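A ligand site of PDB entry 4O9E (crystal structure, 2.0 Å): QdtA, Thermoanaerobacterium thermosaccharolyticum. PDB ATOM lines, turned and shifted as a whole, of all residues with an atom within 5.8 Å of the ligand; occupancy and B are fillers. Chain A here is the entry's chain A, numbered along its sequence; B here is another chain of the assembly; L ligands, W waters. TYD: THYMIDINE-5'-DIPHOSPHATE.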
ATOM      1  N   ARG A  35      -6.164 -22.014  -2.043  1.00  0.00           N
ATOM      2  CA  ARG A  35      -6.806 -22.007  -3.343  1.00  0.00           C
ATOM      3  C   ARG A  35      -7.152 -23.456  -3.656  1.00  0.00           C
ATOM      4  O   ARG A  35      -6.347 -24.346  -3.351  1.00  0.00           O
ATOM      5  CB  ARG A  35      -5.856 -21.483  -4.408  1.00  0.00           C
ATOM      6  CG  ARG A  35      -6.367 -21.775  -5.810  1.00  0.00           C
ATOM      7  CD  ARG A  35      -5.582 -21.022  -6.867  1.00  0.00           C
ATOM      8  NE  ARG A  35      -4.149 -21.272  -6.707  1.00  0.00           N
ATOM      9  CZ  ARG A  35      -3.330 -21.747  -7.638  1.00  0.00           C
ATOM     10  NH1 ARG A  35      -2.050 -21.926  -7.374  1.00  0.00           N
ATOM     11  NH2 ARG A  35      -3.747 -22.073  -8.857  1.00  0.00           N
ATOM     12  N   VAL A  36      -8.343 -23.653  -4.228  1.00  0.00           N
ATOM     13  CA  VAL A  36      -8.714 -24.916  -4.860  1.00  0.00           C
ATOM     14  C   VAL A  36      -9.165 -24.536  -6.266  1.00  0.00           C
ATOM     15  O   VAL A  36      -9.560 -23.399  -6.560  1.00  0.00           O
ATOM     16  CB  VAL A  36      -9.853 -25.680  -4.151  1.00  0.00           C
ATOM     17  CG1 VAL A  36      -9.640 -25.803  -2.648  1.00  0.00           C
ATOM     18  CG2 VAL A  36     -11.142 -24.914  -4.353  1.00  0.00           C
ATOM     19  N   TYR A  37      -8.959 -25.471  -7.169  1.00  0.00           N
ATOM     20  CA  TYR A  37      -9.538 -25.365  -8.499  1.00  0.00           C
ATOM     21  C   TYR A  37      -9.885 -26.761  -8.975  1.00  0.00           C
ATOM     22  O   TYR A  37      -9.382 -27.775  -8.499  1.00  0.00           O
ATOM     23  CB  TYR A  37      -8.597 -24.651  -9.463  1.00  0.00           C
ATOM     24  CG  TYR A  37      -7.275 -25.301  -9.798  1.00  0.00           C
ATOM     25  CD1 TYR A  37      -7.178 -26.167 -10.866  1.00  0.00           C
ATOM     26  CD2 TYR A  37      -6.119 -25.029  -9.085  1.00  0.00           C
ATOM     27  CE1 TYR A  37      -5.975 -26.745 -11.211  1.00  0.00           C
ATOM     28  CE2 TYR A  37      -4.910 -25.648  -9.389  1.00  0.00           C
ATOM     29  CZ  TYR A  37      -4.846 -26.512 -10.473  1.00  0.00           C
ATOM     30  OH  TYR A  37      -3.681 -27.123 -10.886  1.00  0.00           O
ATOM     31  N   ILE A  39     -11.088 -29.128 -12.596  1.00  0.00           N
ATOM     32  CA  ILE A  39     -11.148 -29.305 -14.043  1.00  0.00           C
ATOM     33  C   ILE A  39     -12.195 -30.331 -14.407  1.00  0.00           C
ATOM     34  O   ILE A  39     -12.226 -31.395 -13.816  1.00  0.00           O
ATOM     35  CB  ILE A  39      -9.785 -29.795 -14.535  1.00  0.00           C
ATOM     36  CG1 ILE A  39      -8.770 -28.706 -14.172  1.00  0.00           C
ATOM     37  CG2 ILE A  39      -9.825 -30.080 -16.036  1.00  0.00           C
ATOM     38  CD1 ILE A  39      -7.310 -29.055 -14.371  1.00  0.00           C
ATOM     39  N   ARG A  48      -3.526 -31.973 -20.959  1.00  0.00           N
ATOM     40  CA  ARG A  48      -3.547 -30.753 -20.174  1.00  0.00           C
ATOM     41  C   ARG A  48      -2.230 -30.770 -19.436  1.00  0.00           C
ATOM     42  O   ARG A  48      -1.568 -31.811 -19.373  1.00  0.00           O
ATOM     43  CB  ARG A  48      -4.691 -30.797 -19.175  1.00  0.00           C
ATOM     44  CG  ARG A  48      -6.032 -30.421 -19.808  1.00  0.00           C
ATOM     45  CD  ARG A  48      -7.058 -30.056 -18.757  1.00  0.00           C
ATOM     46  NE  ARG A  48      -6.688 -28.792 -18.111  1.00  0.00           N
ATOM     47  CZ  ARG A  48      -7.300 -27.627 -18.284  1.00  0.00           C
ATOM     48  NH1 ARG A  48      -6.844 -26.550 -17.646  1.00  0.00           N
ATOM     49  NH2 ARG A  48      -8.343 -27.519 -19.097  1.00  0.00           N
ATOM     50  N   GLY A  49      -1.806 -29.626 -18.911  1.00  0.00           N
ATOM     51  CA  GLY A  49      -0.541 -29.597 -18.207  1.00  0.00           C
ATOM     52  C   GLY A  49       0.616 -29.025 -18.989  1.00  0.00           C
ATOM     53  O   GLY A  49       0.561 -27.921 -19.530  1.00  0.00           O
ATOM     54  N   TYR A  50       1.740 -29.737 -18.952  1.00  0.00           N
ATOM     55  CA  TYR A  50       2.979 -29.278 -19.586  1.00  0.00           C
ATOM     56  C   TYR A  50       3.575 -28.109 -18.812  1.00  0.00           C
ATOM     57  O   TYR A  50       3.811 -27.008 -19.325  1.00  0.00           O
ATOM     58  CB  TYR A  50       2.752 -28.867 -21.040  1.00  0.00           C
ATOM     59  CG  TYR A  50       2.160 -29.948 -21.922  1.00  0.00           C
ATOM     60  CD1 TYR A  50       2.941 -31.001 -22.389  1.00  0.00           C
ATOM     61  CD2 TYR A  50       0.828 -29.891 -22.323  1.00  0.00           C
ATOM     62  CE1 TYR A  50       2.416 -31.984 -23.209  1.00  0.00           C
ATOM     63  CE2 TYR A  50       0.286 -30.848 -23.161  1.00  0.00           C
ATOM     64  CZ  TYR A  50       1.094 -31.890 -23.593  1.00  0.00           C
ATOM     65  OH  TYR A  50       0.589 -32.861 -24.421  1.00  0.00           O
ATOM     66  N   HIS A  51       3.811 -28.359 -17.545  1.00  0.00           N
ATOM     67  CA  HIS A  51       4.490 -27.356 -16.738  1.00  0.00           C
ATOM     68  C   HIS A  51       4.884 -27.975 -15.423  1.00  0.00           C
ATOM     69  O   HIS A  51       4.509 -29.098 -15.088  1.00  0.00           O
ATOM     70  CB  HIS A  51       3.597 -26.152 -16.487  1.00  0.00           C
ATOM     71  CG  HIS A  51       2.229 -26.491 -15.967  1.00  0.00           C
ATOM     72  ND1 HIS A  51       2.021 -26.967 -14.700  1.00  0.00           N
ATOM     73  CD2 HIS A  51       1.011 -26.328 -16.527  1.00  0.00           C
ATOM     74  CE1 HIS A  51       0.725 -27.094 -14.485  1.00  0.00           C
ATOM     75  NE2 HIS A  51       0.087 -26.730 -15.587  1.00  0.00           N
ATOM     76  N   ARG A  97       4.477 -31.920 -15.036  1.00  0.00           N
ATOM     77  CA  ARG A  97       3.376 -32.840 -15.234  1.00  0.00           C
ATOM     78  C   ARG A  97       2.507 -32.619 -16.460  1.00  0.00           C
ATOM     79  O   ARG A  97       2.361 -31.502 -16.932  1.00  0.00           O
ATOM     80  CB  ARG A  97       2.475 -32.881 -14.017  1.00  0.00           C
ATOM     81  CG  ARG A  97       1.715 -31.591 -13.744  1.00  0.00           C
ATOM     82  CD  ARG A  97       0.611 -31.936 -12.764  1.00  0.00           C
ATOM     83  NE  ARG A  97      -0.370 -30.858 -12.658  1.00  0.00           N
ATOM     84  CZ  ARG A  97      -0.127 -29.726 -12.037  1.00  0.00           C
ATOM     85  NH1 ARG A  97       1.068 -29.581 -11.459  1.00  0.00           N
ATOM     86  NH2 ARG A  97      -1.085 -28.808 -11.978  1.00  0.00           N
ATOM     87  N   MET A  99      -1.473 -34.204 -17.940  1.00  0.00           N
ATOM     88  CA  MET A  99      -2.650 -34.955 -17.531  1.00  0.00           C
ATOM     89  C   MET A  99      -3.425 -35.388 -18.782  1.00  0.00           C
ATOM     90  O   MET A  99      -3.617 -34.601 -19.719  1.00  0.00           O
ATOM     91  CB  MET A  99      -3.527 -34.080 -16.642  1.00  0.00           C
ATOM     92  CG  MET A  99      -2.745 -33.564 -15.436  1.00  0.00           C
ATOM     93  SD  MET A  99      -2.178 -31.866 -15.655  1.00  0.00           S
ATOM     94  CE  MET A  99      -3.742 -31.097 -15.216  1.00  0.00           C
ATOM     95  N   TYR A 116      -3.015 -18.325  -7.234  1.00  0.00           N
ATOM     96  CA  TYR A 116      -2.461 -18.391  -8.596  1.00  0.00           C
ATOM     97  C   TYR A 116      -1.403 -17.337  -8.882  1.00  0.00           C
ATOM     98  O   TYR A 116      -1.567 -16.177  -8.527  1.00  0.00           O
ATOM     99  CB  TYR A 116      -3.599 -18.173  -9.579  1.00  0.00           C
ATOM    100  CG  TYR A 116      -3.186 -18.134 -11.032  1.00  0.00           C
ATOM    101  CD1 TYR A 116      -2.778 -19.269 -11.733  1.00  0.00           C
ATOM    102  CD2 TYR A 116      -3.273 -16.931 -11.718  1.00  0.00           C
ATOM    103  CE1 TYR A 116      -2.470 -19.196 -13.071  1.00  0.00           C
ATOM    104  CE2 TYR A 116      -2.974 -16.853 -13.057  1.00  0.00           C
ATOM    105  CZ  TYR A 116      -2.555 -17.983 -13.722  1.00  0.00           C
ATOM    106  OH  TYR A 116      -2.256 -17.772 -15.060  1.00  0.00           O
ATOM    107  N   GLU A 118       1.178 -16.727 -12.121  1.00  0.00           N
ATOM    108  CA  GLU A 118       1.660 -17.226 -13.412  1.00  0.00           C
ATOM    109  C   GLU A 118       3.182 -17.221 -13.425  1.00  0.00           C
ATOM    110  O   GLU A 118       3.791 -18.044 -14.097  1.00  0.00           O
ATOM    111  CB  GLU A 118       1.052 -16.479 -14.601  1.00  0.00           C
ATOM    112  CG  GLU A 118       1.480 -17.018 -15.960  1.00  0.00           C
ATOM    113  CD  GLU A 118       1.125 -18.475 -16.231  1.00  0.00           C
ATOM    114  OE1 GLU A 118       1.954 -19.148 -16.885  1.00  0.00           O
ATOM    115  OE2 GLU A 118       0.038 -18.964 -15.818  1.00  0.00           O
ATOM    116  N   TYR A 121       5.020 -20.615 -12.474  1.00  0.00           N
ATOM    117  CA  TYR A 121       4.923 -21.741 -13.414  1.00  0.00           C
ATOM    118  C   TYR A 121       6.219 -21.823 -14.197  1.00  0.00           C
ATOM    119  O   TYR A 121       6.799 -20.782 -14.484  1.00  0.00           O
ATOM    120  CB  TYR A 121       3.861 -21.546 -14.492  1.00  0.00           C
ATOM    121  CG  TYR A 121       2.447 -21.902 -14.114  1.00  0.00           C
ATOM    122  CD1 TYR A 121       1.754 -21.092 -13.229  1.00  0.00           C
ATOM    123  CD2 TYR A 121       1.768 -22.938 -14.732  1.00  0.00           C
ATOM    124  CE1 TYR A 121       0.436 -21.339 -12.924  1.00  0.00           C
ATOM    125  CE2 TYR A 121       0.438 -23.189 -14.448  1.00  0.00           C
ATOM    126  CZ  TYR A 121      -0.214 -22.384 -13.533  1.00  0.00           C
ATOM    127  OH  TYR A 121      -1.523 -22.592 -13.182  1.00  0.00           O
ATOM    128  N   ARG A 123       6.711 -23.218 -17.863  1.00  0.00           N
ATOM    129  CA  ARG A 123       5.983 -23.770 -19.001  1.00  0.00           C
ATOM    130  C   ARG A 123       6.909 -24.125 -20.177  1.00  0.00           C
ATOM    131  O   ARG A 123       6.518 -24.810 -21.117  1.00  0.00           O
ATOM    132  CB  ARG A 123       4.959 -22.742 -19.467  1.00  0.00           C
ATOM    133  CG  ARG A 123       3.903 -22.368 -18.424  1.00  0.00           C
ATOM    134  CD  ARG A 123       2.869 -21.474 -19.069  1.00  0.00           C
ATOM    135  NE  ARG A 123       1.705 -21.210 -18.237  1.00  0.00           N
ATOM    136  CZ  ARG A 123       0.672 -22.018 -18.004  1.00  0.00           C
ATOM    137  NH1 ARG A 123       0.622 -23.271 -18.453  1.00  0.00           N
ATOM    138  NH2 ARG A 123      -0.332 -21.561 -17.260  1.00  0.00           N
ATOM    139  N   LYS B  11     -15.305 -17.810 -11.856  1.00  0.00           N
ATOM    140  CA  LYS B  11     -14.793 -17.865 -13.205  1.00  0.00           C
ATOM    141  C   LYS B  11     -14.897 -19.290 -13.709  1.00  0.00           C
ATOM    142  O   LYS B  11     -14.764 -20.257 -12.954  1.00  0.00           O
ATOM    143  CB  LYS B  11     -13.300 -17.525 -13.225  1.00  0.00           C
ATOM    144  CG  LYS B  11     -13.044 -16.120 -12.723  1.00  0.00           C
ATOM    145  CD  LYS B  11     -11.934 -16.090 -11.688  1.00  0.00           C
ATOM    146  CE  LYS B  11     -10.637 -15.524 -12.218  1.00  0.00           C
ATOM    147  NZ  LYS B  11      -9.805 -15.143 -11.054  1.00  0.00           N
ATOM    148  N   ILE B  13     -12.969 -20.979 -16.862  1.00  0.00           N
ATOM    149  CA  ILE B  13     -11.944 -20.806 -17.883  1.00  0.00           C
ATOM    150  C   ILE B  13     -12.036 -22.017 -18.799  1.00  0.00           C
ATOM    151  O   ILE B  13     -11.638 -23.144 -18.456  1.00  0.00           O
ATOM    152  CB  ILE B  13     -10.537 -20.675 -17.286  1.00  0.00           C
ATOM    153  CG1 ILE B  13     -10.564 -19.464 -16.351  1.00  0.00           C
ATOM    154  CG2 ILE B  13      -9.516 -20.542 -18.403  1.00  0.00           C
ATOM    155  CD1 ILE B  13      -9.669 -19.568 -15.135  1.00  0.00           C
ATOM    156  N   LEU B  20     -12.106 -25.068 -16.257  1.00  0.00           N
ATOM    157  CA  LEU B  20     -11.272 -24.911 -15.063  1.00  0.00           C
ATOM    158  C   LEU B  20     -11.876 -23.740 -14.291  1.00  0.00           C
ATOM    159  O   LEU B  20     -12.079 -22.672 -14.866  1.00  0.00           O
ATOM    160  CB  LEU B  20      -9.793 -24.691 -15.397  1.00  0.00           C
ATOM    161  CG  LEU B  20      -8.908 -24.652 -14.140  1.00  0.00           C
ATOM    162  CD1 LEU B  20      -7.462 -24.918 -14.540  1.00  0.00           C
ATOM    163  CD2 LEU B  20      -8.939 -23.339 -13.400  1.00  0.00           C
ATOM    164  N   PRO B  22     -11.170 -21.800 -10.679  1.00  0.00           N
ATOM    165  CA  PRO B  22     -10.363 -21.610  -9.488  1.00  0.00           C
ATOM    166  C   PRO B  22     -11.167 -20.825  -8.439  1.00  0.00           C
ATOM    167  O   PRO B  22     -12.033 -19.999  -8.768  1.00  0.00           O
ATOM    168  CB  PRO B  22      -9.219 -20.757 -10.015  1.00  0.00           C
ATOM    169  CG  PRO B  22      -9.923 -19.846 -10.967  1.00  0.00           C
ATOM    170  CD  PRO B  22     -11.126 -20.575 -11.507  1.00  0.00           C
ATOM    171  N   GLU B  24     -10.132 -18.846  -4.817  1.00  0.00           N
ATOM    172  CA  GLU B  24      -9.119 -18.430  -3.866  1.00  0.00           C
ATOM    173  C   GLU B  24      -9.800 -17.950  -2.585  1.00  0.00           C
ATOM    174  O   GLU B  24     -10.693 -17.089  -2.612  1.00  0.00           O
ATOM    175  CB  GLU B  24      -8.238 -17.346  -4.486  1.00  0.00           C
ATOM    176  CG  GLU B  24      -7.425 -17.866  -5.675  1.00  0.00           C
ATOM    177  CD  GLU B  24      -6.494 -16.861  -6.349  1.00  0.00           C
ATOM    178  OE1 GLU B  24      -6.699 -15.646  -6.229  1.00  0.00           O
ATOM    179  OE2 GLU B  24      -5.518 -17.276  -7.013  1.00  0.00           O
HETATM  180  PA  TYD L   1      -3.145 -24.157 -16.445  1.00  0.00           P
HETATM  181  O1A TYD L   1      -2.301 -23.435 -17.455  1.00  0.00           O
HETATM  182  O2A TYD L   1      -2.724 -24.312 -14.992  1.00  0.00           O
HETATM  183  O3A TYD L   1      -3.938 -25.490 -16.894  1.00  0.00           O
HETATM  184  PB  TYD L   1      -3.481 -27.040 -16.855  1.00  0.00           P
HETATM  185  O1B TYD L   1      -3.123 -27.284 -18.309  1.00  0.00           O
HETATM  186  O2B TYD L   1      -4.744 -27.721 -16.440  1.00  0.00           O
HETATM  187  O3B TYD L   1      -2.330 -27.200 -15.877  1.00  0.00           O
HETATM  188  O5' TYD L   1      -4.362 -23.127 -16.560  1.00  0.00           O
HETATM  189  C5' TYD L   1      -5.233 -22.833 -17.645  1.00  0.00           C
HETATM  190  C4' TYD L   1      -5.659 -21.375 -17.454  1.00  0.00           C
HETATM  191  O4' TYD L   1      -6.374 -21.114 -16.250  1.00  0.00           O
HETATM  192  C3' TYD L   1      -4.467 -20.439 -17.384  1.00  0.00           C
HETATM  193  O3' TYD L   1      -4.780 -19.383 -18.286  1.00  0.00           O
HETATM  194  C2' TYD L   1      -4.429 -19.772 -16.015  1.00  0.00           C
HETATM  195  C1' TYD L   1      -5.836 -20.020 -15.491  1.00  0.00           C
HETATM  196  N1  TYD L   1      -5.848 -20.309 -14.061  1.00  0.00           N
HETATM  197  C2  TYD L   1      -6.316 -19.437 -13.164  1.00  0.00           C
HETATM  198  O2  TYD L   1      -6.797 -18.354 -13.540  1.00  0.00           O
HETATM  199  N3  TYD L   1      -6.387 -19.743 -11.854  1.00  0.00           N
HETATM  200  C4  TYD L   1      -5.846 -20.891 -11.414  1.00  0.00           C
HETATM  201  O4  TYD L   1      -5.827 -21.118 -10.189  1.00  0.00           O
HETATM  202  C5  TYD L   1      -5.307 -21.799 -12.313  1.00  0.00           C
HETATM  203  C5M TYD L   1      -4.774 -23.137 -11.903  1.00  0.00           C
HETATM  204  C6  TYD L   1      -5.342 -21.482 -13.669  1.00  0.00           C
HETATM  205  O   HOH W   1      -3.512 -28.289 -13.500  1.00  0.00           O
HETATM  206  O   HOH W   2      -1.106 -25.868 -19.544  1.00  0.00           O
HETATM  207  O   HOH W   3      -7.909 -16.106 -13.122  1.00  0.00           O
HETATM  208  O   HOH W   4      -5.119 -26.603 -20.713  1.00  0.00           O
HETATM  209  O   HOH W   5      -7.245 -17.857  -9.803  1.00  0.00           O
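An oxygen (O3B) of the ligand sits at hydrogen-bond distance from a ring nitrogen (NE2) of His 51, at 2.5 Å. The guanidinium group (NH2) of Arg 35 lies within hydrogen-bond range of an oxygen (O4) of the ligand (2.6 Å). O2B of the ligand lies within salt-bridge range of NH1 of Arg 48 (2.7 Å). The guanidinium group (NH2) of Arg 123 is in salt-bridge range of an oxygen (O1A) of the ligand (2.7 Å). N of Gly 49 lies within hydrogen-bond range of O1B of the ligand (2.8 Å). O2A of the ligand sits at hydrogen-bond distance from OH of Tyr 121.
CE2 of Tyr 37 touches C5M of the ligand, at 3.6 Å. CD1 of Ile 39 touches O2B of the ligand (3.6 Å). Met 99 touches the ligand. Tyr 116 touches the ligand. CD1 of Ile 13 of chain B touches O2 of the ligand, at 3.5 Å. Pro 22 of chain B touches the ligand (CB to O4, 3.4 Å). Hydrophobic or aromatic side chains that line the ligand: Tyr 37, Ile 39, His 51, Met 99, Tyr 116, Tyr 121, Ile 13 of chain B and Pro 22 of chain B. Within 4 Å of the ligand: Arg 35, Tyr 37, Ile 39, Arg 48, Gly 49, His 51, Met 99, Tyr 116, Tyr 121, Arg 123, Ile 13 of chain B and Pro 22 of chain B. Along chain A the residues within 4 Å of the ligand span positions 35 to 123.
The backbone NH (N) of Arg 97 is in hydrogen-bond range of the backbone carbonyl oxygen (O) of His 51. The backbone carbonyl oxygen (O) of Arg 48 sits at hydrogen-bond distance from the backbone NH (N) of Met 99 (2.8 Å). NE of Arg 123 lies within salt-bridge range of OE1 of Glu 118 (2.5 Å). The side-chain hydroxyl (OH) of Tyr 116 sits at hydrogen-bond distance from the side-chain carboxylate (OE2) of Glu 118, 2.7 Å away. The side-chain carboxylate of Glu 24 of chain B is in hydrogen-bond range of the backbone NH of Tyr 116, at 2.7 Å. N of Ile 13 of chain B sits at hydrogen-bond distance from O of Leu 20 of chain B. The side-chain hydroxyl of Tyr 37 lies within hydrogen-bond range of the guanidinium group of Arg 97, 3.3 Å away. SD of Met 99 lies within hydrogen-bond range of NE of Arg 97.
Water W3 lies within hydrogen-bond range of an oxygen (O2) of the ligand (2.5 Å) and the side-chain amino group (NZ) of Lys 11 of chain B (3.0 Å). Water W2 lies within hydrogen-bond range of O of Gly 49 (2.6 Å), O1B of the ligand (2.8 Å) and NH1 of Arg 123 (3.3 Å). Water W1 lies within hydrogen-bond range of the side-chain hydroxyl of Tyr 37 (2.9 Å), an oxygen (O3B) of the ligand (2.9 Å) and the guanidinium group of Arg 97 (2.9 Å). Water W5 lies within hydrogen-bond range of N3 of the ligand and OE2 of Glu 24 of chain B.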
